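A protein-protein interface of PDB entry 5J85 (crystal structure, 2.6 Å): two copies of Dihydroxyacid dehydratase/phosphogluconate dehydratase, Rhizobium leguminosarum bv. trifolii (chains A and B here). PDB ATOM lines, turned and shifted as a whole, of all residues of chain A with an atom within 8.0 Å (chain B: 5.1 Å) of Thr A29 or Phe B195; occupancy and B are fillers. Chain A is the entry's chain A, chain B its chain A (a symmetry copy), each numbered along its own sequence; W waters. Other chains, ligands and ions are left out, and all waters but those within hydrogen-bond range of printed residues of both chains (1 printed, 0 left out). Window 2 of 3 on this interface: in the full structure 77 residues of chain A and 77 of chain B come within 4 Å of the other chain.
The guanidinium group (NH1) of Arg A37 is in salt-bridge range of the side-chain carboxylate (OE2) of Glu B199 (2.7 Å). The side-chain amino group (NZ) of Lys A41 is in salt-bridge range of the side-chain carboxylate (OE1) of Glu B199.
The backbone carbonyl oxygen (O) of Gly A28 sits at hydrogen-bond distance from the guanidinium group (NH2) of Arg A37 (2.4 Å). The side-chain amino group of Lys A41 is in hydrogen-bond range of a ring nitrogen (ND1) of His A47 (3.1 Å).
Ser B182 touches Thr A29 (OG to O, 3.6 Å). Thr A29 touches Phe B195 (CG2 to CE2, 3.7 Å). Arg A31 touches Ser B182. Ile A34 touches Phe B195. Glu B199 touches Ile A34 (OE2 to CG2, 2.8 Å). Leu B196 touches His A47 (CD2 to CD2, 3.8 Å).
Of the printed residues of chain B, Ile A34 touches Phe B195 and Glu B199. Printed residues of chain B within 4 Å of Arg A37: Glu B199. Ala B193 touches none of the printed residues of chain A. Phe B195 touches just these residues of chain A: Thr A29 and Ile A34. Of the printed residues of chain A, Leu B196 touches His A47 (3.8 Å). The nearest residue of chain B that does not touch Thr A29 is Val B185 (4.1 Å). The nearest residue of chain A that does not touch Phe B195 is Arg A37 (4.4 Å).
Of the 13 printed residues of chain A, 6 touch a printed residue of chain B. Printed residues of chain A that touch a printed residue of chain B: Thr A29, Arg A31, Ile A34, Arg A37, Lys A41 and His A47. Of the 13 printed residues of chain B, 4 touch a printed residue of chain A. Among the printed residues, 8 pairs touch across the chains. Among the printed residues, Asp or Glu carboxylates within 4 Å of a Lys or Arg side-chain nitrogen of the other chain: Arg A37 with Glu B199 and Lys A41 with Glu B199.
No position is printed for both chains.
Water W1 lies within hydrogen-bond range of the side-chain amino group (NZ) of Lys A41 (2.8 Å) and the backbone carbonyl oxygen (O) of Leu B196 (3.1 Å).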
ATOM      1  N   TYR A  26      -9.388  14.681 -15.130  1.00  0.00           N
ATOM      2  CA  TYR A  26      -9.740  14.652 -13.715  1.00  0.00           C
ATOM      3  C   TYR A  26     -10.882  15.592 -13.337  1.00  0.00           C
ATOM      4  O   TYR A  26     -11.172  15.743 -12.139  1.00  0.00           O
ATOM      5  CB  TYR A  26      -8.508  14.994 -12.865  1.00  0.00           C
ATOM      6  CG  TYR A  26      -7.376  13.996 -12.968  1.00  0.00           C
ATOM      7  CD1 TYR A  26      -7.633  12.631 -13.087  1.00  0.00           C
ATOM      8  CD2 TYR A  26      -6.051  14.417 -12.944  1.00  0.00           C
ATOM      9  CE1 TYR A  26      -6.603  11.712 -13.176  1.00  0.00           C
ATOM     10  CE2 TYR A  26      -5.009  13.505 -13.030  1.00  0.00           C
ATOM     11  CZ  TYR A  26      -5.291  12.148 -13.144  1.00  0.00           C
ATOM     12  OH  TYR A  26      -4.265  11.231 -13.232  1.00  0.00           O
ATOM     13  N   GLY A  27     -11.530  16.234 -14.306  1.00  0.00           N
ATOM     14  CA  GLY A  27     -12.533  17.252 -14.032  1.00  0.00           C
ATOM     15  C   GLY A  27     -13.918  16.812 -14.477  1.00  0.00           C
ATOM     16  O   GLY A  27     -14.116  16.410 -15.632  1.00  0.00           O
ATOM     17  N   GLY A  28     -14.866  16.898 -13.551  1.00  0.00           N
ATOM     18  CA  GLY A  28     -16.255  16.609 -13.829  1.00  0.00           C
ATOM     19  C   GLY A  28     -16.743  15.347 -13.145  1.00  0.00           C
ATOM     20  O   GLY A  28     -16.189  14.882 -12.146  1.00  0.00           O
ATOM     21  N   THR A  29     -17.825  14.790 -13.699  1.00  0.00           N
ATOM     22  CA  THR A  29     -18.411  13.569 -13.159  1.00  0.00           C
ATOM     23  C   THR A  29     -18.812  12.575 -14.244  1.00  0.00           C
ATOM     24  O   THR A  29     -19.488  11.586 -13.930  1.00  0.00           O
ATOM     25  CB  THR A  29     -19.636  13.878 -12.275  1.00  0.00           C
ATOM     26  OG1 THR A  29     -20.367  14.979 -12.832  1.00  0.00           O
ATOM     27  CG2 THR A  29     -19.211  14.214 -10.842  1.00  0.00           C
ATOM     28  N   SER A  30     -18.430  12.807 -15.500  1.00  0.00           N
ATOM     29  CA  SER A  30     -18.632  11.810 -16.541  1.00  0.00           C
ATOM     30  C   SER A  30     -17.911  10.515 -16.169  1.00  0.00           C
ATOM     31  O   SER A  30     -16.975  10.505 -15.359  1.00  0.00           O
ATOM     32  CB  SER A  30     -18.138  12.332 -17.893  1.00  0.00           C
ATOM     33  OG  SER A  30     -16.734  12.553 -17.886  1.00  0.00           O
ATOM     34  N   ARG A  31     -18.376   9.401 -16.754  1.00  0.00           N
ATOM     35  CA  ARG A  31     -17.725   8.124 -16.483  1.00  0.00           C
ATOM     36  C   ARG A  31     -16.247   8.191 -16.824  1.00  0.00           C
ATOM     37  O   ARG A  31     -15.425   7.691 -16.049  1.00  0.00           O
ATOM     38  CB  ARG A  31     -18.446   6.983 -17.245  1.00  0.00           C
ATOM     39  CG  ARG A  31     -17.849   5.525 -17.164  1.00  0.00           C
ATOM     40  CD  ARG A  31     -16.492   5.312 -17.845  1.00  0.00           C
ATOM     41  NE  ARG A  31     -16.620   5.400 -19.278  1.00  0.00           N
ATOM     42  CZ  ARG A  31     -17.194   4.505 -20.063  1.00  0.00           C
ATOM     43  NH1 ARG A  31     -17.647   3.360 -19.587  1.00  0.00           N
ATOM     44  NH2 ARG A  31     -17.251   4.764 -21.357  1.00  0.00           N
ATOM     45  N   ASP A  32     -15.892   8.874 -17.913  1.00  0.00           N
ATOM     46  CA  ASP A  32     -14.487   8.974 -18.296  1.00  0.00           C
ATOM     47  C   ASP A  32     -13.626   9.461 -17.137  1.00  0.00           C
ATOM     48  O   ASP A  32     -12.543   8.918 -16.885  1.00  0.00           O
ATOM     49  CB  ASP A  32     -14.326   9.897 -19.501  1.00  0.00           C
ATOM     50  CG  ASP A  32     -13.327   9.355 -20.492  1.00  0.00           C
ATOM     51  OD1 ASP A  32     -12.146   9.211 -20.106  1.00  0.00           O
ATOM     52  OD2 ASP A  32     -13.735   9.003 -21.624  1.00  0.00           O
ATOM     53  N   VAL A  33     -14.127  10.434 -16.376  1.00  0.00           N
ATOM     54  CA  VAL A  33     -13.307  11.078 -15.361  1.00  0.00           C
ATOM     55  C   VAL A  33     -13.287  10.285 -14.043  1.00  0.00           C
ATOM     56  O   VAL A  33     -12.280  10.302 -13.325  1.00  0.00           O
ATOM     57  CB  VAL A  33     -13.793  12.530 -15.200  1.00  0.00           C
ATOM     58  CG1 VAL A  33     -13.230  13.176 -13.945  1.00  0.00           C
ATOM     59  CG2 VAL A  33     -13.422  13.335 -16.454  1.00  0.00           C
ATOM     60  N   ILE A  34     -14.350   9.547 -13.706  1.00  0.00           N
ATOM     61  CA  ILE A  34     -14.280   8.769 -12.467  1.00  0.00           C
ATOM     62  C   ILE A  34     -13.441   7.506 -12.662  1.00  0.00           C
ATOM     63  O   ILE A  34     -12.904   6.965 -11.682  1.00  0.00           O
ATOM     64  CB  ILE A  34     -15.688   8.468 -11.903  1.00  0.00           C
ATOM     65  CG1 ILE A  34     -16.694   8.030 -12.967  1.00  0.00           C
ATOM     66  CG2 ILE A  34     -16.260   9.697 -11.220  1.00  0.00           C
ATOM     67  CD1 ILE A  34     -16.515   6.635 -13.438  1.00  0.00           C
ATOM     68  N   TYR A  35     -13.293   7.033 -13.902  1.00  0.00           N
ATOM     69  CA  TYR A  35     -12.271   6.036 -14.197  1.00  0.00           C
ATOM     70  C   TYR A  35     -10.883   6.595 -13.896  1.00  0.00           C
ATOM     71  O   TYR A  35     -10.158   6.072 -13.042  1.00  0.00           O
ATOM     72  CB  TYR A  35     -12.382   5.592 -15.661  1.00  0.00           C
ATOM     73  CG  TYR A  35     -11.293   4.637 -16.139  1.00  0.00           C
ATOM     74  CD1 TYR A  35     -11.066   3.421 -15.495  1.00  0.00           C
ATOM     75  CD2 TYR A  35     -10.509   4.944 -17.252  1.00  0.00           C
ATOM     76  CE1 TYR A  35     -10.077   2.544 -15.938  1.00  0.00           C
ATOM     77  CE2 TYR A  35      -9.521   4.073 -17.703  1.00  0.00           C
ATOM     78  CZ  TYR A  35      -9.311   2.876 -17.041  1.00  0.00           C
ATOM     79  OH  TYR A  35      -8.337   2.009 -17.482  1.00  0.00           O
ATOM     80  N   ARG A  37      -9.853   9.517 -12.431  1.00  0.00           N
ATOM     81  CA  ARG A  37      -9.658  10.052 -11.086  1.00  0.00           C
ATOM     82  C   ARG A  37      -9.736   8.946 -10.038  1.00  0.00           C
ATOM     83  O   ARG A  37      -8.902   8.882  -9.124  1.00  0.00           O
ATOM     84  CB  ARG A  37     -10.694  11.151 -10.809  1.00  0.00           C
ATOM     85  CG  ARG A  37     -10.541  11.850  -9.475  1.00  0.00           C
ATOM     86  CD  ARG A  37     -11.890  12.263  -8.901  1.00  0.00           C
ATOM     87  NE  ARG A  37     -12.511  13.313  -9.701  1.00  0.00           N
ATOM     88  CZ  ARG A  37     -13.730  13.254 -10.223  1.00  0.00           C
ATOM     89  NH1 ARG A  37     -14.506  12.194 -10.037  1.00  0.00           N
ATOM     90  NH2 ARG A  37     -14.173  14.269 -10.942  1.00  0.00           N
ATOM     91  N   LYS A  41      -6.791   7.536  -7.290  1.00  0.00           N
ATOM     92  CA  LYS A  41      -7.074   7.624  -5.862  1.00  0.00           C
ATOM     93  C   LYS A  41      -6.665   6.376  -5.088  1.00  0.00           C
ATOM     94  O   LYS A  41      -6.709   6.393  -3.847  1.00  0.00           O
ATOM     95  CB  LYS A  41      -8.561   7.898  -5.647  1.00  0.00           C
ATOM     96  CG  LYS A  41      -8.996   9.321  -6.001  1.00  0.00           C
ATOM     97  CD  LYS A  41     -10.400   9.589  -5.490  1.00  0.00           C
ATOM     98  CE  LYS A  41     -10.866  11.001  -5.780  1.00  0.00           C
ATOM     99  NZ  LYS A  41     -12.213  11.236  -5.185  1.00  0.00           N
ATOM    100  N   HIS A  47      -9.476  14.318  -2.291  1.00  0.00           N
ATOM    101  CA  HIS A  47     -10.231  14.583  -3.516  1.00  0.00           C
ATOM    102  C   HIS A  47      -9.954  15.976  -4.076  1.00  0.00           C
ATOM    103  O   HIS A  47      -9.995  16.170  -5.298  1.00  0.00           O
ATOM    104  CB  HIS A  47     -11.734  14.409  -3.279  1.00  0.00           C
ATOM    105  CG  HIS A  47     -12.577  14.891  -4.423  1.00  0.00           C
ATOM    106  ND1 HIS A  47     -12.635  14.232  -5.636  1.00  0.00           N
ATOM    107  CD2 HIS A  47     -13.370  15.983  -4.552  1.00  0.00           C
ATOM    108  CE1 HIS A  47     -13.436  14.891  -6.458  1.00  0.00           C
ATOM    109  NE2 HIS A  47     -13.896  15.956  -5.824  1.00  0.00           N
ATOM    110  N   PHE B 181     -22.963   4.772 -10.705  1.00  0.00           N
ATOM    111  CA  PHE B 181     -22.579   5.953  -9.931  1.00  0.00           C
ATOM    112  C   PHE B 181     -22.561   7.220 -10.776  1.00  0.00           C
ATOM    113  O   PHE B 181     -22.736   8.316 -10.234  1.00  0.00           O
ATOM    114  CB  PHE B 181     -21.212   5.748  -9.268  1.00  0.00           C
ATOM    115  CG  PHE B 181     -21.171   4.594  -8.300  1.00  0.00           C
ATOM    116  CD1 PHE B 181     -22.346   4.024  -7.819  1.00  0.00           C
ATOM    117  CD2 PHE B 181     -19.957   4.070  -7.878  1.00  0.00           C
ATOM    118  CE1 PHE B 181     -22.314   2.957  -6.940  1.00  0.00           C
ATOM    119  CE2 PHE B 181     -19.917   3.003  -6.998  1.00  0.00           C
ATOM    120  CZ  PHE B 181     -21.099   2.443  -6.533  1.00  0.00           C
ATOM    121  N   SER B 182     -22.353   7.096 -12.092  1.00  0.00           N
ATOM    122  CA  SER B 182     -22.506   8.254 -12.971  1.00  0.00           C
ATOM    123  C   SER B 182     -23.975   8.521 -13.280  1.00  0.00           C
ATOM    124  O   SER B 182     -24.397   9.680 -13.371  1.00  0.00           O
ATOM    125  CB  SER B 182     -21.715   8.047 -14.267  1.00  0.00           C
ATOM    126  OG  SER B 182     -21.820   9.177 -15.125  1.00  0.00           O
ATOM    127  N   VAL B 185     -25.316  10.273 -10.025  1.00  0.00           N
ATOM    128  CA  VAL B 185     -24.859  11.613  -9.663  1.00  0.00           C
ATOM    129  C   VAL B 185     -25.639  12.671 -10.440  1.00  0.00           C
ATOM    130  O   VAL B 185     -25.859  13.784  -9.941  1.00  0.00           O
ATOM    131  CB  VAL B 185     -23.336  11.750  -9.873  1.00  0.00           C
ATOM    132  CG1 VAL B 185     -22.957  11.553 -11.340  1.00  0.00           C
ATOM    133  CG2 VAL B 185     -22.834  13.102  -9.356  1.00  0.00           C
ATOM    134  N   MET B 190     -28.227  10.392  -5.470  1.00  0.00           N
ATOM    135  CA  MET B 190     -27.234  10.438  -4.404  1.00  0.00           C
ATOM    136  C   MET B 190     -26.561  11.809  -4.380  1.00  0.00           C
ATOM    137  O   MET B 190     -26.423  12.470  -5.414  1.00  0.00           O
ATOM    138  CB  MET B 190     -26.187   9.314  -4.542  1.00  0.00           C
ATOM    139  CG  MET B 190     -25.212   9.433  -5.714  1.00  0.00           C
ATOM    140  SD  MET B 190     -24.143   7.977  -5.877  1.00  0.00           S
ATOM    141  CE  MET B 190     -23.583   7.780  -4.188  1.00  0.00           C
ATOM    142  N   THR B 191     -26.157  12.218  -3.176  1.00  0.00           N
ATOM    143  CA  THR B 191     -25.450  13.468  -2.921  1.00  0.00           C
ATOM    144  C   THR B 191     -24.167  13.535  -3.758  1.00  0.00           C
ATOM    145  O   THR B 191     -23.803  12.594  -4.468  1.00  0.00           O
ATOM    146  CB  THR B 191     -25.105  13.570  -1.429  1.00  0.00           C
ATOM    147  OG1 THR B 191     -26.201  13.081  -0.649  1.00  0.00           O
ATOM    148  CG2 THR B 191     -24.818  15.012  -0.999  1.00  0.00           C
ATOM    149  N   GLN B 192     -23.481  14.683  -3.679  1.00  0.00           N
ATOM    150  CA  GLN B 192     -22.089  14.734  -4.113  1.00  0.00           C
ATOM    151  C   GLN B 192     -21.150  14.244  -3.014  1.00  0.00           C
ATOM    152  O   GLN B 192     -20.115  13.638  -3.318  1.00  0.00           O
ATOM    153  CB  GLN B 192     -21.708  16.154  -4.563  1.00  0.00           C
ATOM    154  CG  GLN B 192     -21.347  17.134  -3.439  1.00  0.00           C
ATOM    155  CD  GLN B 192     -19.854  17.470  -3.383  1.00  0.00           C
ATOM    156  OE1 GLN B 192     -19.193  17.609  -4.417  1.00  0.00           O
ATOM    157  NE2 GLN B 192     -19.323  17.603  -2.169  1.00  0.00           N
ATOM    158  N   ALA B 193     -21.500  14.469  -1.741  1.00  0.00           N
ATOM    159  CA  ALA B 193     -20.716  13.897  -0.651  1.00  0.00           C
ATOM    160  C   ALA B 193     -20.917  12.389  -0.551  1.00  0.00           C
ATOM    161  O   ALA B 193     -20.030  11.682  -0.065  1.00  0.00           O
ATOM    162  CB  ALA B 193     -21.069  14.577   0.673  1.00  0.00           C
ATOM    163  N   GLU B 194     -22.072  11.880  -1.000  1.00  0.00           N
ATOM    164  CA  GLU B 194     -22.263  10.437  -1.125  1.00  0.00           C
ATOM    165  C   GLU B 194     -21.447   9.864  -2.278  1.00  0.00           C
ATOM    166  O   GLU B 194     -20.962   8.730  -2.193  1.00  0.00           O
ATOM    167  CB  GLU B 194     -23.745  10.105  -1.342  1.00  0.00           C
ATOM    168  CG  GLU B 194     -24.626  10.105  -0.093  1.00  0.00           C
ATOM    169  CD  GLU B 194     -26.042   9.613  -0.386  1.00  0.00           C
ATOM    170  OE1 GLU B 194     -26.671   9.028   0.519  1.00  0.00           O
ATOM    171  OE2 GLU B 194     -26.523   9.805  -1.523  1.00  0.00           O
ATOM    172  N   PHE B 195     -21.296  10.629  -3.361  1.00  0.00           N
ATOM    173  CA  PHE B 195     -20.624  10.151  -4.565  1.00  0.00           C
ATOM    174  C   PHE B 195     -19.114  10.070  -4.389  1.00  0.00           C
ATOM    175  O   PHE B 195     -18.464   9.213  -5.002  1.00  0.00           O
ATOM    176  CB  PHE B 195     -20.965  11.071  -5.737  1.00  0.00           C
ATOM    177  CG  PHE B 195     -20.247  10.732  -7.008  1.00  0.00           C
ATOM    178  CD1 PHE B 195     -20.551   9.565  -7.693  1.00  0.00           C
ATOM    179  CD2 PHE B 195     -19.287  11.587  -7.531  1.00  0.00           C
ATOM    180  CE1 PHE B 195     -19.906   9.250  -8.867  1.00  0.00           C
ATOM    181  CE2 PHE B 195     -18.641  11.273  -8.706  1.00  0.00           C
ATOM    182  CZ  PHE B 195     -18.955  10.104  -9.374  1.00  0.00           C
ATOM    183  N   LEU B 196     -18.541  10.954  -3.573  1.00  0.00           N
ATOM    184  CA  LEU B 196     -17.103  10.927  -3.343  1.00  0.00           C
ATOM    185  C   LEU B 196     -16.701   9.749  -2.458  1.00  0.00           C
ATOM    186  O   LEU B 196     -15.602   9.206  -2.625  1.00  0.00           O
ATOM    187  CB  LEU B 196     -16.649  12.260  -2.741  1.00  0.00           C
ATOM    188  CG  LEU B 196     -16.463  13.457  -3.687  1.00  0.00           C
ATOM    189  CD1 LEU B 196     -17.489  13.484  -4.817  1.00  0.00           C
ATOM    190  CD2 LEU B 196     -16.515  14.757  -2.888  1.00  0.00           C
ATOM    191  N   GLU B 197     -17.570   9.331  -1.523  1.00  0.00           N
ATOM    192  CA  GLU B 197     -17.321   8.086  -0.796  1.00  0.00           C
ATOM    193  C   GLU B 197     -17.446   6.870  -1.706  1.00  0.00           C
ATOM    194  O   GLU B 197     -16.730   5.883  -1.510  1.00  0.00           O
ATOM    195  CB  GLU B 197     -18.270   7.926   0.402  1.00  0.00           C
ATOM    196  CG  GLU B 197     -18.693   9.209   1.114  1.00  0.00           C
ATOM    197  CD  GLU B 197     -19.944   9.018   1.985  1.00  0.00           C
ATOM    198  OE1 GLU B 197     -20.663   8.008   1.796  1.00  0.00           O
ATOM    199  OE2 GLU B 197     -20.217   9.891   2.843  1.00  0.00           O
ATOM    200  N   ALA B 198     -18.340   6.922  -2.702  1.00  0.00           N
ATOM    201  CA  ALA B 198     -18.521   5.793  -3.613  1.00  0.00           C
ATOM    202  C   ALA B 198     -17.290   5.573  -4.489  1.00  0.00           C
ATOM    203  O   ALA B 198     -16.844   4.432  -4.676  1.00  0.00           O
ATOM    204  CB  ALA B 198     -19.757   6.017  -4.485  1.00  0.00           C
ATOM    205  N   GLU B 199     -16.744   6.654  -5.049  1.00  0.00           N
ATOM    206  CA  GLU B 199     -15.555   6.553  -5.885  1.00  0.00           C
ATOM    207  C   GLU B 199     -14.357   6.068  -5.079  1.00  0.00           C
ATOM    208  O   GLU B 199     -13.553   5.263  -5.565  1.00  0.00           O
ATOM    209  CB  GLU B 199     -15.268   7.916  -6.508  1.00  0.00           C
ATOM    210  CG  GLU B 199     -14.565   7.874  -7.832  1.00  0.00           C
ATOM    211  CD  GLU B 199     -14.063   9.243  -8.231  1.00  0.00           C
ATOM    212  OE1 GLU B 199     -13.548   9.979  -7.356  1.00  0.00           O
ATOM    213  OE2 GLU B 199     -14.175   9.586  -9.420  1.00  0.00           O
HETATM  214  O   HOH W   1     -13.082  10.971  -2.513  1.00  0.00           O
